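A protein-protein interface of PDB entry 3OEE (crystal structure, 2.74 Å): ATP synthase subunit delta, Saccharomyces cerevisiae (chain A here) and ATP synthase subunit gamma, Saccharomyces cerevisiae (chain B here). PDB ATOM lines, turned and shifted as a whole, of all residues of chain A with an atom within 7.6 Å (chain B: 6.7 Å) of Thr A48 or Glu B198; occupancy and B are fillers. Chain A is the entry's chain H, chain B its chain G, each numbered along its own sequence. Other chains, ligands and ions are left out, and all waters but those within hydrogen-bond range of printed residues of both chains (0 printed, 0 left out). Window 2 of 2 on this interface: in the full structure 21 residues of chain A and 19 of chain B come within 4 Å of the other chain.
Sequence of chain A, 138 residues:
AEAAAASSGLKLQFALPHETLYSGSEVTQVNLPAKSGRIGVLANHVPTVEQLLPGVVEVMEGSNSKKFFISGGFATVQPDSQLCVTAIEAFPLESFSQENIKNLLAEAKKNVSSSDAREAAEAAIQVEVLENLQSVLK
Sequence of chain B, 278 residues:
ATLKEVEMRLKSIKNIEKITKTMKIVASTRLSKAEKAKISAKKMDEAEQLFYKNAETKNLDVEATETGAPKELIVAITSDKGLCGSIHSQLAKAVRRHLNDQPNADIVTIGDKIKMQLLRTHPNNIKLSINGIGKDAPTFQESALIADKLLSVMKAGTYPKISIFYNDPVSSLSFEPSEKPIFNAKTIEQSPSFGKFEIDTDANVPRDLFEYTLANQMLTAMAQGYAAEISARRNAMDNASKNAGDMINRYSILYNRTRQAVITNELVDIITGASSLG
Of the 8 printed residues of chain B, 4 touch a printed residue of chain A.
Printed residues of chain B that touch a printed residue of chain A: Lys B196, Phe B197, Glu B198 and Ile B199.
Among the printed residues, 8 pairs touch across the chains.
Among the printed residues, no Asp or Glu carboxylate lies within 4 Å of a Lys or Arg side-chain nitrogen of the other chain.
O of Pro A47 lies within hydrogen-bond range of N of Glu B198.
Pro A47 touches Lys B196.
Pro A47 touches Phe B197.
OG1 of Thr A48 touches CB of Glu B198, at 3.4 Å.
O of Val A49 touches CA of Ile B199 (3.9 Å).
Phe B197 touches Val A77 (CE1 to O, 3.5 Å).
Gln A78 touches Phe B197 (OE1 to CE1, 3.5 Å).
Pro A79 touches Phe B197.
Printed residues of chain B within 4 Å of Pro A47: Lys B196 (3.95 Å), Phe B197 (3.4 Å) and Glu B198 (2.9 Å).
Thr A48 touches just one residue of chain B: Glu B198 (3.4 Å).
Printed residues of chain B within 4 Å of Val A77: Phe B197.
Of chain A, only Pro A47 (2.9 Å) and Thr A48 (3.4 Å) come within 4 Å of Glu B198.
Of the printed residues of chain A, Ile B199 touches Val A49.
The nearest residue of chain A that does not touch Glu B198 is Val A46 (4.2 Å).
O of Val A46 lies within hydrogen-bond range of OG1 of Thr A48 (3.1 Å).
O of Thr A48 lies within hydrogen-bond range of N of Val A77 (2.7 Å).
OG1 of Thr A76 sits at hydrogen-bond distance from OE1 of Gln A78, 2.7 Å away.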
ATOM      1  N   LYS A  35      33.710  18.109  25.913  1.00  0.00           N
ATOM      2  CA  LYS A  35      34.330  19.402  26.241  1.00  0.00           C
ATOM      3  C   LYS A  35      34.969  19.384  27.630  1.00  0.00           C
ATOM      4  O   LYS A  35      36.172  19.613  27.770  1.00  0.00           O
ATOM      5  CB  LYS A  35      33.312  20.555  26.119  1.00  0.00           C
ATOM      6  CG  LYS A  35      32.006  20.408  26.924  1.00  0.00           C
ATOM      7  CD  LYS A  35      30.964  19.609  26.159  1.00  0.00           C
ATOM      8  CE  LYS A  35      29.782  19.249  27.035  1.00  0.00           C
ATOM      9  NZ  LYS A  35      28.925  18.249  26.343  1.00  0.00           N
ATOM     10  N   ILE A  39      29.313  12.736  28.610  1.00  0.00           N
ATOM     11  CA  ILE A  39      27.965  12.454  28.110  1.00  0.00           C
ATOM     12  C   ILE A  39      27.715  10.951  27.923  1.00  0.00           C
ATOM     13  O   ILE A  39      28.561  10.228  27.396  1.00  0.00           O
ATOM     14  CB  ILE A  39      27.664  13.284  26.802  1.00  0.00           C
ATOM     15  CG1 ILE A  39      26.892  14.586  27.126  1.00  0.00           C
ATOM     16  CG2 ILE A  39      26.960  12.446  25.717  1.00  0.00           C
ATOM     17  CD1 ILE A  39      25.402  14.425  27.514  1.00  0.00           C
ATOM     18  N   HIS A  45      18.764  11.294  21.326  1.00  0.00           N
ATOM     19  CA  HIS A  45      19.475  12.525  21.670  1.00  0.00           C
ATOM     20  C   HIS A  45      19.412  13.538  20.537  1.00  0.00           C
ATOM     21  O   HIS A  45      19.611  13.196  19.364  1.00  0.00           O
ATOM     22  CB  HIS A  45      20.934  12.237  22.067  1.00  0.00           C
ATOM     23  CG  HIS A  45      21.593  13.349  22.832  1.00  0.00           C
ATOM     24  ND1 HIS A  45      20.986  13.995  23.888  1.00  0.00           N
ATOM     25  CD2 HIS A  45      22.824  13.905  22.712  1.00  0.00           C
ATOM     26  CE1 HIS A  45      21.804  14.913  24.373  1.00  0.00           C
ATOM     27  NE2 HIS A  45      22.928  14.877  23.679  1.00  0.00           N
ATOM     28  N   VAL A  46      19.108  14.778  20.911  1.00  0.00           N
ATOM     29  CA  VAL A  46      19.180  15.928  20.017  1.00  0.00           C
ATOM     30  C   VAL A  46      20.604  16.048  19.467  1.00  0.00           C
ATOM     31  O   VAL A  46      21.563  16.073  20.244  1.00  0.00           O
ATOM     32  CB  VAL A  46      18.756  17.239  20.756  1.00  0.00           C
ATOM     33  CG1 VAL A  46      19.380  18.489  20.126  1.00  0.00           C
ATOM     34  CG2 VAL A  46      17.237  17.363  20.795  1.00  0.00           C
ATOM     35  N   PRO A  47      20.744  16.081  18.124  1.00  0.00           N
ATOM     36  CA  PRO A  47      22.027  16.331  17.466  1.00  0.00           C
ATOM     37  C   PRO A  47      22.890  17.384  18.182  1.00  0.00           C
ATOM     38  O   PRO A  47      22.437  18.503  18.438  1.00  0.00           O
ATOM     39  CB  PRO A  47      21.613  16.813  16.069  1.00  0.00           C
ATOM     40  CG  PRO A  47      20.248  16.218  15.836  1.00  0.00           C
ATOM     41  CD  PRO A  47      19.706  15.698  17.148  1.00  0.00           C
ATOM     42  N   THR A  48      24.117  16.995  18.518  1.00  0.00           N
ATOM     43  CA  THR A  48      25.058  17.852  19.236  1.00  0.00           C
ATOM     44  C   THR A  48      26.480  17.496  18.828  1.00  0.00           C
ATOM     45  O   THR A  48      26.816  16.320  18.684  1.00  0.00           O
ATOM     46  CB  THR A  48      24.900  17.714  20.770  1.00  0.00           C
ATOM     47  OG1 THR A  48      23.608  18.195  21.160  1.00  0.00           O
ATOM     48  CG2 THR A  48      25.968  18.512  21.517  1.00  0.00           C
ATOM     49  N   VAL A  49      27.301  18.525  18.643  1.00  0.00           N
ATOM     50  CA  VAL A  49      28.709  18.368  18.290  1.00  0.00           C
ATOM     51  C   VAL A  49      29.590  18.850  19.446  1.00  0.00           C
ATOM     52  O   VAL A  49      29.477  19.992  19.892  1.00  0.00           O
ATOM     53  CB  VAL A  49      29.038  19.128  16.978  1.00  0.00           C
ATOM     54  CG1 VAL A  49      30.535  19.198  16.733  1.00  0.00           C
ATOM     55  CG2 VAL A  49      28.347  18.467  15.807  1.00  0.00           C
ATOM     56  N   GLU A  50      30.452  17.964  19.939  1.00  0.00           N
ATOM     57  CA  GLU A  50      31.402  18.302  21.005  1.00  0.00           C
ATOM     58  C   GLU A  50      32.735  17.564  20.844  1.00  0.00           C
ATOM     59  O   GLU A  50      32.773  16.372  20.511  1.00  0.00           O
ATOM     60  CB  GLU A  50      30.798  18.035  22.390  1.00  0.00           C
ATOM     61  N   ALA A  75      33.098  14.142  18.502  1.00  0.00           N
ATOM     62  CA  ALA A  75      31.882  13.353  18.628  1.00  0.00           C
ATOM     63  C   ALA A  75      30.725  14.183  18.111  1.00  0.00           C
ATOM     64  O   ALA A  75      30.557  15.338  18.512  1.00  0.00           O
ATOM     65  CB  ALA A  75      31.649  12.965  20.065  1.00  0.00           C
ATOM     66  N   THR A  76      29.943  13.608  17.204  1.00  0.00           N
ATOM     67  CA  THR A  76      28.798  14.313  16.634  1.00  0.00           C
ATOM     68  C   THR A  76      27.524  13.458  16.692  1.00  0.00           C
ATOM     69  O   THR A  76      27.456  12.381  16.087  1.00  0.00           O
ATOM     70  CB  THR A  76      29.060  14.813  15.172  1.00  0.00           C
ATOM     71  OG1 THR A  76      28.614  13.834  14.230  1.00  0.00           O
ATOM     72  CG2 THR A  76      30.545  15.114  14.917  1.00  0.00           C
ATOM     73  N   VAL A  77      26.533  13.929  17.448  1.00  0.00           N
ATOM     74  CA  VAL A  77      25.195  13.353  17.413  1.00  0.00           C
ATOM     75  C   VAL A  77      24.548  13.952  16.178  1.00  0.00           C
ATOM     76  O   VAL A  77      24.580  15.167  15.994  1.00  0.00           O
ATOM     77  CB  VAL A  77      24.364  13.723  18.665  1.00  0.00           C
ATOM     78  CG1 VAL A  77      23.098  12.867  18.752  1.00  0.00           C
ATOM     79  CG2 VAL A  77      25.192  13.585  19.934  1.00  0.00           C
ATOM     80  N   GLN A  78      23.977  13.106  15.329  1.00  0.00           N
ATOM     81  CA  GLN A  78      23.501  13.545  14.012  1.00  0.00           C
ATOM     82  C   GLN A  78      21.963  13.677  13.933  1.00  0.00           C
ATOM     83  O   GLN A  78      21.262  13.250  14.856  1.00  0.00           O
ATOM     84  CB  GLN A  78      24.044  12.616  12.912  1.00  0.00           C
ATOM     85  CG  GLN A  78      25.566  12.359  12.946  1.00  0.00           C
ATOM     86  CD  GLN A  78      26.412  13.552  12.495  1.00  0.00           C
ATOM     87  OE1 GLN A  78      26.303  14.657  13.038  1.00  0.00           O
ATOM     88  NE2 GLN A  78      27.286  13.319  11.518  1.00  0.00           N
ATOM     89  N   PRO A  79      21.439  14.306  12.851  1.00  0.00           N
ATOM     90  CA  PRO A  79      19.990  14.404  12.598  1.00  0.00           C
ATOM     91  C   PRO A  79      19.279  13.060  12.403  1.00  0.00           C
ATOM     92  O   PRO A  79      18.073  12.963  12.649  1.00  0.00           O
ATOM     93  CB  PRO A  79      19.920  15.241  11.317  1.00  0.00           C
ATOM     94  CG  PRO A  79      21.124  16.101  11.393  1.00  0.00           C
ATOM     95  CD  PRO A  79      22.191  15.194  11.944  1.00  0.00           C
ATOM     96  N   GLN A  82      21.763   9.056  15.154  1.00  0.00           N
ATOM     97  CA  GLN A  82      22.918   8.188  15.372  1.00  0.00           C
ATOM     98  C   GLN A  82      24.065   8.981  15.999  1.00  0.00           C
ATOM     99  O   GLN A  82      24.079  10.215  15.938  1.00  0.00           O
ATOM    100  CB  GLN A  82      23.370   7.550  14.052  1.00  0.00           C
ATOM    101  N   LEU A  83      25.011   8.275  16.616  1.00  0.00           N
ATOM    102  CA  LEU A  83      26.208   8.913  17.154  1.00  0.00           C
ATOM    103  C   LEU A  83      27.388   8.686  16.220  1.00  0.00           C
ATOM    104  O   LEU A  83      27.438   7.691  15.498  1.00  0.00           O
ATOM    105  CB  LEU A  83      26.536   8.390  18.560  1.00  0.00           C
ATOM    106  CG  LEU A  83      27.849   8.863  19.209  1.00  0.00           C
ATOM    107  CD1 LEU A  83      27.809  10.344  19.578  1.00  0.00           C
ATOM    108  CD2 LEU A  83      28.190   8.031  20.422  1.00  0.00           C
ATOM    109  N   CYS A  84      28.327   9.624  16.234  1.00  0.00           N
ATOM    110  CA  CYS A  84      29.582   9.469  15.518  1.00  0.00           C
ATOM    111  C   CYS A  84      30.758   9.872  16.398  1.00  0.00           C
ATOM    112  O   CYS A  84      30.830  11.010  16.873  1.00  0.00           O
ATOM    113  CB  CYS A  84      29.574  10.275  14.215  1.00  0.00           C
ATOM    114  SG  CYS A  84      28.442   9.624  12.946  1.00  0.00           S
ATOM    115  N   PHE B 194      23.268  25.773  11.168  1.00  0.00           N
ATOM    116  CA  PHE B 194      24.170  25.617  12.308  1.00  0.00           C
ATOM    117  C   PHE B 194      23.360  25.294  13.555  1.00  0.00           C
ATOM    118  O   PHE B 194      23.867  24.679  14.498  1.00  0.00           O
ATOM    119  CB  PHE B 194      25.016  26.871  12.534  1.00  0.00           C
ATOM    120  CG  PHE B 194      26.172  26.663  13.474  1.00  0.00           C
ATOM    121  CD1 PHE B 194      27.127  25.677  13.220  1.00  0.00           C
ATOM    122  CD2 PHE B 194      26.317  27.458  14.605  1.00  0.00           C
ATOM    123  CE1 PHE B 194      28.205  25.480  14.087  1.00  0.00           C
ATOM    124  CE2 PHE B 194      27.386  27.274  15.477  1.00  0.00           C
ATOM    125  CZ  PHE B 194      28.334  26.283  15.220  1.00  0.00           C
ATOM    126  N   GLY B 195      22.092  25.705  13.524  1.00  0.00           N
ATOM    127  CA  GLY B 195      21.173  25.584  14.653  1.00  0.00           C
ATOM    128  C   GLY B 195      20.530  24.220  14.794  1.00  0.00           C
ATOM    129  O   GLY B 195      19.952  23.913  15.838  1.00  0.00           O
ATOM    130  N   LYS B 196      20.620  23.405  13.743  1.00  0.00           N
ATOM    131  CA  LYS B 196      20.203  22.005  13.825  1.00  0.00           C
ATOM    132  C   LYS B 196      20.919  21.300  14.978  1.00  0.00           C
ATOM    133  O   LYS B 196      20.307  20.525  15.710  1.00  0.00           O
ATOM    134  CB  LYS B 196      20.444  21.266  12.502  1.00  0.00           C
ATOM    135  CG  LYS B 196      19.369  21.526  11.452  1.00  0.00           C
ATOM    136  CD  LYS B 196      18.987  20.263  10.686  1.00  0.00           C
ATOM    137  CE  LYS B 196      19.713  20.145   9.360  1.00  0.00           C
ATOM    138  NZ  LYS B 196      19.184  19.020   8.540  1.00  0.00           N
ATOM    139  N   PHE B 197      22.206  21.607  15.143  1.00  0.00           N
ATOM    140  CA  PHE B 197      23.042  21.023  16.195  1.00  0.00           C
ATOM    141  C   PHE B 197      23.130  21.927  17.426  1.00  0.00           C
ATOM    142  O   PHE B 197      23.192  23.154  17.305  1.00  0.00           O
ATOM    143  CB  PHE B 197      24.445  20.703  15.651  1.00  0.00           C
ATOM    144  CG  PHE B 197      24.436  19.800  14.441  1.00  0.00           C
ATOM    145  CD1 PHE B 197      24.393  18.416  14.589  1.00  0.00           C
ATOM    146  CD2 PHE B 197      24.459  20.333  13.152  1.00  0.00           C
ATOM    147  CE1 PHE B 197      24.373  17.578  13.477  1.00  0.00           C
ATOM    148  CE2 PHE B 197      24.440  19.499  12.031  1.00  0.00           C
ATOM    149  CZ  PHE B 197      24.398  18.120  12.198  1.00  0.00           C
ATOM    150  N   GLU B 198      23.136  21.309  18.607  1.00  0.00           N
ATOM    151  CA  GLU B 198      23.176  22.047  19.867  1.00  0.00           C
ATOM    152  C   GLU B 198      24.617  22.255  20.332  1.00  0.00           C
ATOM    153  O   GLU B 198      24.925  22.132  21.518  1.00  0.00           O
ATOM    154  CB  GLU B 198      22.337  21.331  20.937  1.00  0.00           C
ATOM    155  CG  GLU B 198      21.910  22.204  22.131  1.00  0.00           C
ATOM    156  CD  GLU B 198      20.908  23.303  21.771  1.00  0.00           C
ATOM    157  OE1 GLU B 198      20.243  23.211  20.715  1.00  0.00           O
ATOM    158  OE2 GLU B 198      20.777  24.264  22.560  1.00  0.00           O
ATOM    159  N   ILE B 199      25.490  22.576  19.379  1.00  0.00           N
ATOM    160  CA  ILE B 199      26.890  22.882  19.661  1.00  0.00           C
ATOM    161  C   ILE B 199      27.005  23.973  20.728  1.00  0.00           C
ATOM    162  O   ILE B 199      26.281  24.972  20.686  1.00  0.00           O
ATOM    163  CB  ILE B 199      27.640  23.329  18.389  1.00  0.00           C
ATOM    164  N   ASP B 200      27.896  23.759  21.694  1.00  0.00           N
ATOM    165  CA  ASP B 200      28.175  24.749  22.729  1.00  0.00           C
ATOM    166  C   ASP B 200      28.969  25.899  22.121  1.00  0.00           C
ATOM    167  O   ASP B 200      30.045  25.688  21.562  1.00  0.00           O
ATOM    168  CB  ASP B 200      28.948  24.114  23.885  1.00  0.00           C
ATOM    169  N   THR B 201      28.422  27.108  22.219  1.00  0.00           N
ATOM    170  CA  THR B 201      29.030  28.301  21.620  1.00  0.00           C
ATOM    171  C   THR B 201      29.934  29.034  22.627  1.00  0.00           C
ATOM    172  O   THR B 201      29.723  30.211  22.942  1.00  0.00           O
ATOM    173  CB  THR B 201      27.939  29.242  21.018  1.00  0.00           C
ATOM    174  OG1 THR B 201      28.555  30.406  20.455  1.00  0.00           O
ATOM    175  CG2 THR B 201      26.897  29.663  22.073  1.00  0.00           C
